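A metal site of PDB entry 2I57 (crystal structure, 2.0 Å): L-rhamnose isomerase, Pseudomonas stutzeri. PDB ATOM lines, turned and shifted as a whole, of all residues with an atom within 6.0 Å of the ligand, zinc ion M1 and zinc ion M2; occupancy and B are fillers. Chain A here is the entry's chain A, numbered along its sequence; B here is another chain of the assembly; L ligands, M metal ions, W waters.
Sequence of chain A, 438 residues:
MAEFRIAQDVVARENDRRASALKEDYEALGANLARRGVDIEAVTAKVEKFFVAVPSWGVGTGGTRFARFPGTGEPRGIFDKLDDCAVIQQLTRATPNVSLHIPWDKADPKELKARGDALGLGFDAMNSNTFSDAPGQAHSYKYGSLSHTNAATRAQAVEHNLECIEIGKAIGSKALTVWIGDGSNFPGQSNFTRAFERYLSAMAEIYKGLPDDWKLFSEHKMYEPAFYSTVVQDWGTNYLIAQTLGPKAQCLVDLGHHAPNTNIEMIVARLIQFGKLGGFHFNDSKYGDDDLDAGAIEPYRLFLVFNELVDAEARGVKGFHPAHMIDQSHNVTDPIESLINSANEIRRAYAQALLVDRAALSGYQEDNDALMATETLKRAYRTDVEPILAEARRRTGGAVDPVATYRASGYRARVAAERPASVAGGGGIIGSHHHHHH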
ATOM      1  N   TRP A  57      14.013 -36.008 -21.949  1.00  0.00           N
ATOM      2  CA  TRP A  57      15.311 -35.685 -22.534  1.00  0.00           C
ATOM      3  C   TRP A  57      16.484 -36.493 -21.967  1.00  0.00           C
ATOM      4  O   TRP A  57      17.610 -36.384 -22.463  1.00  0.00           O
ATOM      5  CB  TRP A  57      15.592 -34.190 -22.380  1.00  0.00           C
ATOM      6  CG  TRP A  57      15.716 -33.720 -20.965  1.00  0.00           C
ATOM      7  CD1 TRP A  57      16.865 -33.648 -20.210  1.00  0.00           C
ATOM      8  CD2 TRP A  57      14.654 -33.264 -20.110  1.00  0.00           C
ATOM      9  NE1 TRP A  57      16.577 -33.180 -18.948  1.00  0.00           N
ATOM     10  CE2 TRP A  57      15.233 -32.935 -18.867  1.00  0.00           C
ATOM     11  CE3 TRP A  57      13.279 -33.100 -20.288  1.00  0.00           C
ATOM     12  CZ2 TRP A  57      14.475 -32.444 -17.796  1.00  0.00           C
ATOM     13  CZ3 TRP A  57      12.523 -32.623 -19.217  1.00  0.00           C
ATOM     14  CH2 TRP A  57      13.119 -32.300 -17.989  1.00  0.00           C
ATOM     15  N   HIS A 101       9.575 -31.719 -22.442  1.00  0.00           N
ATOM     16  CA  HIS A 101      10.302 -30.485 -22.712  1.00  0.00           C
ATOM     17  C   HIS A 101       9.852 -29.976 -24.083  1.00  0.00           C
ATOM     18  O   HIS A 101       9.895 -30.722 -25.071  1.00  0.00           O
ATOM     19  CB  HIS A 101      11.804 -30.756 -22.711  1.00  0.00           C
ATOM     20  CG  HIS A 101      12.614 -29.664 -22.092  1.00  0.00           C
ATOM     21  ND1 HIS A 101      12.644 -28.378 -22.588  1.00  0.00           N
ATOM     22  CD2 HIS A 101      13.427 -29.660 -21.008  1.00  0.00           C
ATOM     23  CE1 HIS A 101      13.427 -27.631 -21.829  1.00  0.00           C
ATOM     24  NE2 HIS A 101      13.924 -28.393 -20.864  1.00  0.00           N
ATOM     25  N   TRP A 104      11.195 -29.665 -27.879  1.00  0.00           N
ATOM     26  CA  TRP A 104      11.743 -30.982 -28.209  1.00  0.00           C
ATOM     27  C   TRP A 104      10.673 -32.050 -28.363  1.00  0.00           C
ATOM     28  O   TRP A 104      10.676 -32.816 -29.326  1.00  0.00           O
ATOM     29  CB  TRP A 104      12.746 -31.463 -27.158  1.00  0.00           C
ATOM     30  CG  TRP A 104      13.972 -30.613 -27.040  1.00  0.00           C
ATOM     31  CD1 TRP A 104      14.519 -29.807 -27.991  1.00  0.00           C
ATOM     32  CD2 TRP A 104      14.829 -30.512 -25.889  1.00  0.00           C
ATOM     33  NE1 TRP A 104      15.656 -29.202 -27.506  1.00  0.00           N
ATOM     34  CE2 TRP A 104      15.865 -29.621 -26.219  1.00  0.00           C
ATOM     35  CE3 TRP A 104      14.802 -31.089 -24.606  1.00  0.00           C
ATOM     36  CZ2 TRP A 104      16.877 -29.280 -25.318  1.00  0.00           C
ATOM     37  CZ3 TRP A 104      15.808 -30.756 -23.707  1.00  0.00           C
ATOM     38  CH2 TRP A 104      16.837 -29.861 -24.073  1.00  0.00           C
ATOM     39  N   ASN A 127       8.190 -28.431 -19.227  1.00  0.00           N
ATOM     40  CA  ASN A 127       9.419 -27.655 -19.155  1.00  0.00           C
ATOM     41  C   ASN A 127       9.518 -26.783 -20.394  1.00  0.00           C
ATOM     42  O   ASN A 127       9.431 -27.298 -21.509  1.00  0.00           O
ATOM     43  CB  ASN A 127      10.631 -28.585 -19.081  1.00  0.00           C
ATOM     44  CG  ASN A 127      10.705 -29.351 -17.781  1.00  0.00           C
ATOM     45  OD1 ASN A 127      11.269 -28.871 -16.792  1.00  0.00           O
ATOM     46  ND2 ASN A 127      10.126 -30.547 -17.761  1.00  0.00           N
ATOM     47  N   SER A 128       9.699 -25.478 -20.217  1.00  0.00           N
ATOM     48  CA  SER A 128       9.825 -24.582 -21.355  1.00  0.00           C
ATOM     49  C   SER A 128      11.284 -24.469 -21.787  1.00  0.00           C
ATOM     50  O   SER A 128      12.199 -24.747 -21.009  1.00  0.00           O
ATOM     51  CB  SER A 128       9.256 -23.196 -21.009  1.00  0.00           C
ATOM     52  OG  SER A 128       9.896 -22.667 -19.863  1.00  0.00           O
ATOM     53  N   PHE A 131      16.271 -21.243 -23.946  1.00  0.00           N
ATOM     54  CA  PHE A 131      17.720 -21.186 -23.802  1.00  0.00           C
ATOM     55  C   PHE A 131      18.391 -21.645 -25.109  1.00  0.00           C
ATOM     56  O   PHE A 131      19.605 -21.840 -25.170  1.00  0.00           O
ATOM     57  CB  PHE A 131      18.185 -22.052 -22.604  1.00  0.00           C
ATOM     58  CG  PHE A 131      17.679 -23.473 -22.626  1.00  0.00           C
ATOM     59  CD1 PHE A 131      18.236 -24.423 -23.476  1.00  0.00           C
ATOM     60  CD2 PHE A 131      16.648 -23.866 -21.768  1.00  0.00           C
ATOM     61  CE1 PHE A 131      17.787 -25.740 -23.479  1.00  0.00           C
ATOM     62  CE2 PHE A 131      16.187 -25.178 -21.766  1.00  0.00           C
ATOM     63  CZ  PHE A 131      16.755 -26.111 -22.611  1.00  0.00           C
ATOM     64  N   THR A 177       7.751 -25.830 -15.313  1.00  0.00           N
ATOM     65  CA  THR A 177       9.068 -25.542 -14.759  1.00  0.00           C
ATOM     66  C   THR A 177       9.793 -24.625 -15.712  1.00  0.00           C
ATOM     67  O   THR A 177       9.863 -24.879 -16.921  1.00  0.00           O
ATOM     68  CB  THR A 177       9.914 -26.822 -14.601  1.00  0.00           C
ATOM     69  OG1 THR A 177       9.354 -27.626 -13.557  1.00  0.00           O
ATOM     70  CG2 THR A 177      11.352 -26.478 -14.264  1.00  0.00           C
ATOM     71  N   TRP A 179      13.383 -22.899 -16.465  1.00  0.00           N
ATOM     72  CA  TRP A 179      14.815 -22.750 -16.271  1.00  0.00           C
ATOM     73  C   TRP A 179      15.292 -22.048 -17.521  1.00  0.00           C
ATOM     74  O   TRP A 179      14.972 -22.482 -18.629  1.00  0.00           O
ATOM     75  CB  TRP A 179      15.565 -24.078 -16.159  1.00  0.00           C
ATOM     76  CG  TRP A 179      17.054 -23.818 -16.154  1.00  0.00           C
ATOM     77  CD1 TRP A 179      17.792 -23.255 -15.148  1.00  0.00           C
ATOM     78  CD2 TRP A 179      17.949 -23.977 -17.270  1.00  0.00           C
ATOM     79  NE1 TRP A 179      19.089 -23.047 -15.562  1.00  0.00           N
ATOM     80  CE2 TRP A 179      19.209 -23.475 -16.855  1.00  0.00           C
ATOM     81  CE3 TRP A 179      17.818 -24.479 -18.570  1.00  0.00           C
ATOM     82  CZ2 TRP A 179      20.330 -23.469 -17.708  1.00  0.00           C
ATOM     83  CZ3 TRP A 179      18.923 -24.468 -19.408  1.00  0.00           C
ATOM     84  CH2 TRP A 179      20.161 -23.969 -18.980  1.00  0.00           C
ATOM     85  N   GLU A 219      13.651 -22.355 -11.487  1.00  0.00           N
ATOM     86  CA  GLU A 219      14.846 -23.118 -11.107  1.00  0.00           C
ATOM     87  C   GLU A 219      16.118 -22.288 -11.167  1.00  0.00           C
ATOM     88  O   GLU A 219      16.478 -21.750 -12.213  1.00  0.00           O
ATOM     89  CB  GLU A 219      14.966 -24.329 -12.045  1.00  0.00           C
ATOM     90  CG  GLU A 219      16.238 -25.159 -11.907  1.00  0.00           C
ATOM     91  CD  GLU A 219      16.198 -26.397 -12.798  1.00  0.00           C
ATOM     92  OE1 GLU A 219      15.392 -26.423 -13.747  1.00  0.00           O
ATOM     93  OE2 GLU A 219      16.995 -27.330 -12.561  1.00  0.00           O
ATOM     94  N   LYS A 221      20.302 -21.518 -10.842  1.00  0.00           N
ATOM     95  CA  LYS A 221      21.538 -22.156 -11.273  1.00  0.00           C
ATOM     96  C   LYS A 221      22.654 -21.111 -11.176  1.00  0.00           C
ATOM     97  O   LYS A 221      22.535 -20.012 -11.714  1.00  0.00           O
ATOM     98  CB  LYS A 221      21.415 -22.655 -12.711  1.00  0.00           C
ATOM     99  CG  LYS A 221      22.518 -23.618 -13.128  1.00  0.00           C
ATOM    100  CD  LYS A 221      22.340 -24.092 -14.579  1.00  0.00           C
ATOM    101  CE  LYS A 221      23.456 -25.052 -14.989  1.00  0.00           C
ATOM    102  NZ  LYS A 221      23.307 -25.491 -16.415  1.00  0.00           N
ATOM    103  N   GLU A 224      26.439 -21.366 -16.127  1.00  0.00           N
ATOM    104  CA  GLU A 224      26.291 -22.226 -17.305  1.00  0.00           C
ATOM    105  C   GLU A 224      24.839 -22.232 -17.756  1.00  0.00           C
ATOM    106  O   GLU A 224      23.963 -22.740 -17.064  1.00  0.00           O
ATOM    107  CB  GLU A 224      26.726 -23.683 -17.055  1.00  0.00           C
ATOM    108  CG  GLU A 224      26.642 -24.522 -18.347  1.00  0.00           C
ATOM    109  CD  GLU A 224      26.648 -26.029 -18.140  1.00  0.00           C
ATOM    110  OE1 GLU A 224      26.067 -26.515 -17.137  1.00  0.00           O
ATOM    111  OE2 GLU A 224      27.211 -26.748 -19.000  1.00  0.00           O
ATOM    112  N   ASP A 254      17.744 -27.946  -7.971  1.00  0.00           N
ATOM    113  CA  ASP A 254      18.477 -28.940  -8.754  1.00  0.00           C
ATOM    114  C   ASP A 254      19.817 -29.095  -8.042  1.00  0.00           C
ATOM    115  O   ASP A 254      20.631 -28.171  -8.010  1.00  0.00           O
ATOM    116  CB  ASP A 254      18.698 -28.458 -10.195  1.00  0.00           C
ATOM    117  CG  ASP A 254      19.340 -29.523 -11.078  1.00  0.00           C
ATOM    118  OD1 ASP A 254      20.397 -30.058 -10.685  1.00  0.00           O
ATOM    119  OD2 ASP A 254      18.802 -29.816 -12.169  1.00  0.00           O
ATOM    120  N   HIS A 257      23.177 -27.496  -9.135  1.00  0.00           N
ATOM    121  CA  HIS A 257      23.227 -26.078  -9.475  1.00  0.00           C
ATOM    122  C   HIS A 257      23.731 -25.123  -8.406  1.00  0.00           C
ATOM    123  O   HIS A 257      23.400 -23.941  -8.455  1.00  0.00           O
ATOM    124  CB  HIS A 257      21.834 -25.604  -9.901  1.00  0.00           C
ATOM    125  CG  HIS A 257      21.338 -26.235 -11.162  1.00  0.00           C
ATOM    126  ND1 HIS A 257      20.241 -25.763 -11.850  1.00  0.00           N
ATOM    127  CD2 HIS A 257      21.788 -27.298 -11.868  1.00  0.00           C
ATOM    128  CE1 HIS A 257      20.036 -26.513 -12.918  1.00  0.00           C
ATOM    129  NE2 HIS A 257      20.958 -27.449 -12.954  1.00  0.00           N
ATOM    130  N   HIS A 281      15.147 -31.598  -8.524  1.00  0.00           N
ATOM    131  CA  HIS A 281      15.706 -32.096  -9.762  1.00  0.00           C
ATOM    132  C   HIS A 281      16.871 -32.907  -9.211  1.00  0.00           C
ATOM    133  O   HIS A 281      17.890 -32.354  -8.793  1.00  0.00           O
ATOM    134  CB  HIS A 281      16.202 -30.967 -10.669  1.00  0.00           C
ATOM    135  CG  HIS A 281      15.219 -30.590 -11.737  1.00  0.00           C
ATOM    136  ND1 HIS A 281      15.568 -29.833 -12.835  1.00  0.00           N
ATOM    137  CD2 HIS A 281      13.894 -30.848 -11.876  1.00  0.00           C
ATOM    138  CE1 HIS A 281      14.510 -29.652 -13.604  1.00  0.00           C
ATOM    139  NE2 HIS A 281      13.483 -30.258 -13.039  1.00  0.00           N
ATOM    140  N   ASN A 283      20.034 -35.495  -9.174  1.00  0.00           N
ATOM    141  CA  ASN A 283      21.214 -35.869  -9.939  1.00  0.00           C
ATOM    142  C   ASN A 283      22.381 -35.784  -8.956  1.00  0.00           C
ATOM    143  O   ASN A 283      22.182 -35.504  -7.771  1.00  0.00           O
ATOM    144  CB  ASN A 283      21.425 -34.911 -11.135  1.00  0.00           C
ATOM    145  CG  ASN A 283      21.358 -33.447 -10.745  1.00  0.00           C
ATOM    146  OD1 ASN A 283      22.068 -32.980  -9.844  1.00  0.00           O
ATOM    147  ND2 ASN A 283      20.499 -32.695 -11.435  1.00  0.00           N
ATOM    148  N   ASP A 289      27.621 -28.514 -12.631  1.00  0.00           N
ATOM    149  CA  ASP A 289      26.303 -29.100 -12.901  1.00  0.00           C
ATOM    150  C   ASP A 289      26.598 -30.320 -13.771  1.00  0.00           C
ATOM    151  O   ASP A 289      26.226 -30.385 -14.942  1.00  0.00           O
ATOM    152  CB  ASP A 289      25.419 -28.096 -13.647  1.00  0.00           C
ATOM    153  CG  ASP A 289      24.068 -28.677 -14.019  1.00  0.00           C
ATOM    154  OD1 ASP A 289      23.535 -29.525 -13.273  1.00  0.00           O
ATOM    155  OD2 ASP A 289      23.520 -28.280 -15.077  1.00  0.00           O
ATOM    156  N   ASP A 291      25.375 -33.271 -13.761  1.00  0.00           N
ATOM    157  CA  ASP A 291      24.205 -34.057 -14.147  1.00  0.00           C
ATOM    158  C   ASP A 291      24.440 -35.569 -14.177  1.00  0.00           C
ATOM    159  O   ASP A 291      23.951 -36.262 -15.064  1.00  0.00           O
ATOM    160  CB  ASP A 291      23.671 -33.606 -15.515  1.00  0.00           C
ATOM    161  CG  ASP A 291      23.086 -32.207 -15.483  1.00  0.00           C
ATOM    162  OD1 ASP A 291      22.593 -31.805 -14.417  1.00  0.00           O
ATOM    163  OD2 ASP A 291      23.124 -31.510 -16.516  1.00  0.00           O
ATOM    164  N   ASP A 327      16.792 -35.088 -13.245  1.00  0.00           N
ATOM    165  CA  ASP A 327      17.275 -34.235 -14.333  1.00  0.00           C
ATOM    166  C   ASP A 327      18.741 -34.598 -14.506  1.00  0.00           C
ATOM    167  O   ASP A 327      19.612 -34.047 -13.836  1.00  0.00           O
ATOM    168  CB  ASP A 327      17.148 -32.755 -13.991  1.00  0.00           C
ATOM    169  CG  ASP A 327      17.593 -31.846 -15.138  1.00  0.00           C
ATOM    170  OD1 ASP A 327      18.075 -32.378 -16.160  1.00  0.00           O
ATOM    171  OD2 ASP A 327      17.456 -30.621 -15.009  1.00  0.00           O
ATOM    172  N   ARG B  65      26.776 -26.638 -24.138  1.00  0.00           N
ATOM    173  CA  ARG B  65      26.038 -27.854 -24.433  1.00  0.00           C
ATOM    174  C   ARG B  65      24.556 -27.589 -24.645  1.00  0.00           C
ATOM    175  O   ARG B  65      23.820 -28.459 -25.112  1.00  0.00           O
ATOM    176  CB  ARG B  65      26.224 -28.888 -23.313  1.00  0.00           C
ATOM    177  CG  ARG B  65      25.785 -28.421 -21.944  1.00  0.00           C
ATOM    178  CD  ARG B  65      25.825 -29.572 -20.938  1.00  0.00           C
ATOM    179  NE  ARG B  65      25.668 -29.083 -19.573  1.00  0.00           N
ATOM    180  CZ  ARG B  65      25.080 -29.743 -18.580  1.00  0.00           C
ATOM    181  NH1 ARG B  65      24.572 -30.958 -18.793  1.00  0.00           N
ATOM    182  NH2 ARG B  65      24.971 -29.181 -17.387  1.00  0.00           N
ATOM    183  N   PHE B  66      24.105 -26.383 -24.307  1.00  0.00           N
ATOM    184  CA  PHE B  66      22.708 -26.021 -24.455  1.00  0.00           C
ATOM    185  C   PHE B  66      22.423 -25.337 -25.777  1.00  0.00           C
ATOM    186  O   PHE B  66      21.336 -25.483 -26.342  1.00  0.00           O
ATOM    187  CB  PHE B  66      22.267 -25.103 -23.311  1.00  0.00           C
ATOM    188  CG  PHE B  66      22.335 -25.746 -21.965  1.00  0.00           C
ATOM    189  CD1 PHE B  66      21.338 -26.627 -21.551  1.00  0.00           C
ATOM    190  CD2 PHE B  66      23.406 -25.497 -21.117  1.00  0.00           C
ATOM    191  CE1 PHE B  66      21.418 -27.265 -20.320  1.00  0.00           C
ATOM    192  CE2 PHE B  66      23.499 -26.134 -19.880  1.00  0.00           C
ATOM    193  CZ  PHE B  66      22.506 -27.014 -19.476  1.00  0.00           C
HETATM  194  C1  LIG L   1      19.752 -26.891 -16.787  1.00  0.00           C
HETATM  195  O1  LIG L   1      20.940 -27.008 -16.428  1.00  0.00           O
HETATM  196  C2  LIG L   1      18.635 -27.332 -15.839  1.00  0.00           C
HETATM  197  O2  LIG L   1      18.922 -28.617 -15.309  1.00  0.00           O
HETATM  198  C3  LIG L   1      17.272 -27.333 -16.556  1.00  0.00           C
HETATM  199  O3  LIG L   1      16.337 -28.072 -15.790  1.00  0.00           O
HETATM  200  C4  LIG L   1      17.313 -27.874 -17.988  1.00  0.00           C
HETATM  201  O4  LIG L   1      16.066 -27.629 -18.632  1.00  0.00           O
HETATM  202  C5  LIG L   1      17.615 -29.375 -18.031  1.00  0.00           C
HETATM  203  O5  LIG L   1      18.957 -29.608 -17.650  1.00  0.00           O
HETATM  204  C6  LIG L   1      17.385 -29.906 -19.431  1.00  0.00           C
HETATM  205  O6  LIG L   1      18.213 -29.199 -20.345  1.00  0.00           O
HETATM  206 ZN    ZN M   1      17.228 -29.115 -13.603  1.00  0.00          ZN
HETATM  207 ZN    ZN M   2      21.332 -28.330 -14.808  1.00  0.00          ZN
HETATM  208  O   HOH W   1      13.599 -27.165 -17.260  1.00  0.00           O
HETATM  209  O   HOH W   2      21.488 -29.589 -17.039  1.00  0.00           O
HETATM  210  O   HOH W   3      20.907 -30.127 -14.006  1.00  0.00           O
HETATM  211  O   HOH W   4      20.492 -32.663 -17.690  1.00  0.00           O
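Of the 20 residues printed, 5 come within 4 Å of zinc ion M1.
The nearest printed residue that does not touch zinc ion M1 is Asn 283 (5.3 Å).
A ring nitrogen (NE2) of His 101 lies within hydrogen-bond range of an oxygen (O4) of the ligand.
O1 of the ligand lies close to NZ of Lys 221 (2.8 Å).
Lys 221 touches zinc ion M2 (NZ to ZN, 3.8 Å).
Asp 291 touches zinc ion M2 (OD1 to ZN, 3.7 Å).
Five residues have an atom within 4 Å of zinc ion M2: Lys 221, Asp 254, His 257, Asp 289 and Asp 291.
Along chain A the residues within 4 Å of zinc ion M2 span positions 221 to 291.
OD1 of Asp 291 sits close to OD1 of Asp 289 (2.7 Å).
OD1 of Asp 327 sits at hydrogen-bond distance from NE1 of Trp 57 (3.3 Å).
The side-chain carboxylate (OD1) of Asp 254 is in hydrogen-bond range of the side-chain amide nitrogen (ND2) of Asn 283 (2.7 Å).
NZ of Lys 221 sits close to OD2 of Asp 289 (3.1 Å).
The side-chain amide nitrogen of Asn 283 lies within hydrogen-bond range of the backbone carbonyl oxygen of Asp 327 (2.9 Å).
NZ of Lys 221 lies within salt-bridge range of OE1 of Glu 224, 3.0 Å away.
OD2 of Asp 291 lies within salt-bridge range of NH1 of Arg 65 of chain B (2.8 Å).
O of Asp 289 sits at hydrogen-bond distance from NH2 of Arg 65 of chain B, 3.0 Å away.
Zinc ion M2 is bound by water W3 (2.0 Å), a ring nitrogen (NE2) of His 257 (2.1 Å), an oxygen (O1) of the ligand (2.1 Å), the side-chain carboxylate of Asp 289 (2.2 Å), an oxygen (O2) of the ligand (2.5 Å) and water W2 (2.6 Å).
ND1 of His 281 is bound to zinc ion M1.
Zinc ion M1 is bound by OD2 of Asp 327 (2.1 Å).
OE2 of Glu 219 binds zinc ion M1 (2.1 Å).
Zinc ion M1 is bound by the side-chain carboxylate (OD2) of Asp 254 (2.2 Å).
O2 of the ligand is bound to zinc ion M1.
Zinc ion M1 is bound by O3 of the ligand (2.6 Å).
Merely in contact with the ligand: Trp 57 (3.4 Å), Phe 66 of chain B (3.4 Å), Trp 179 (3.5 Å) and Phe 131 (3.98 Å).
Hydrophobic or aromatic side chains within 4 Å of the ligand: Trp 57, Phe 131, Trp 179, His 257, His 281 and Phe 66 of chain B.
Water W2 lies within hydrogen-bond range of the side-chain carboxylate (OD2) of Asp 291 and an oxygen (O5) of the ligand.
Water W1 lies within hydrogen-bond range of O4 of the ligand (2.9 Å) and OD1 of Asn 127 (2.9 Å).
Water W4 lies within hydrogen-bond range of the side-chain carboxylate (OD1) of Asp 327, the side-chain carboxylate (OD2) of Asp 291 and an oxygen (O5) of the ligand.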
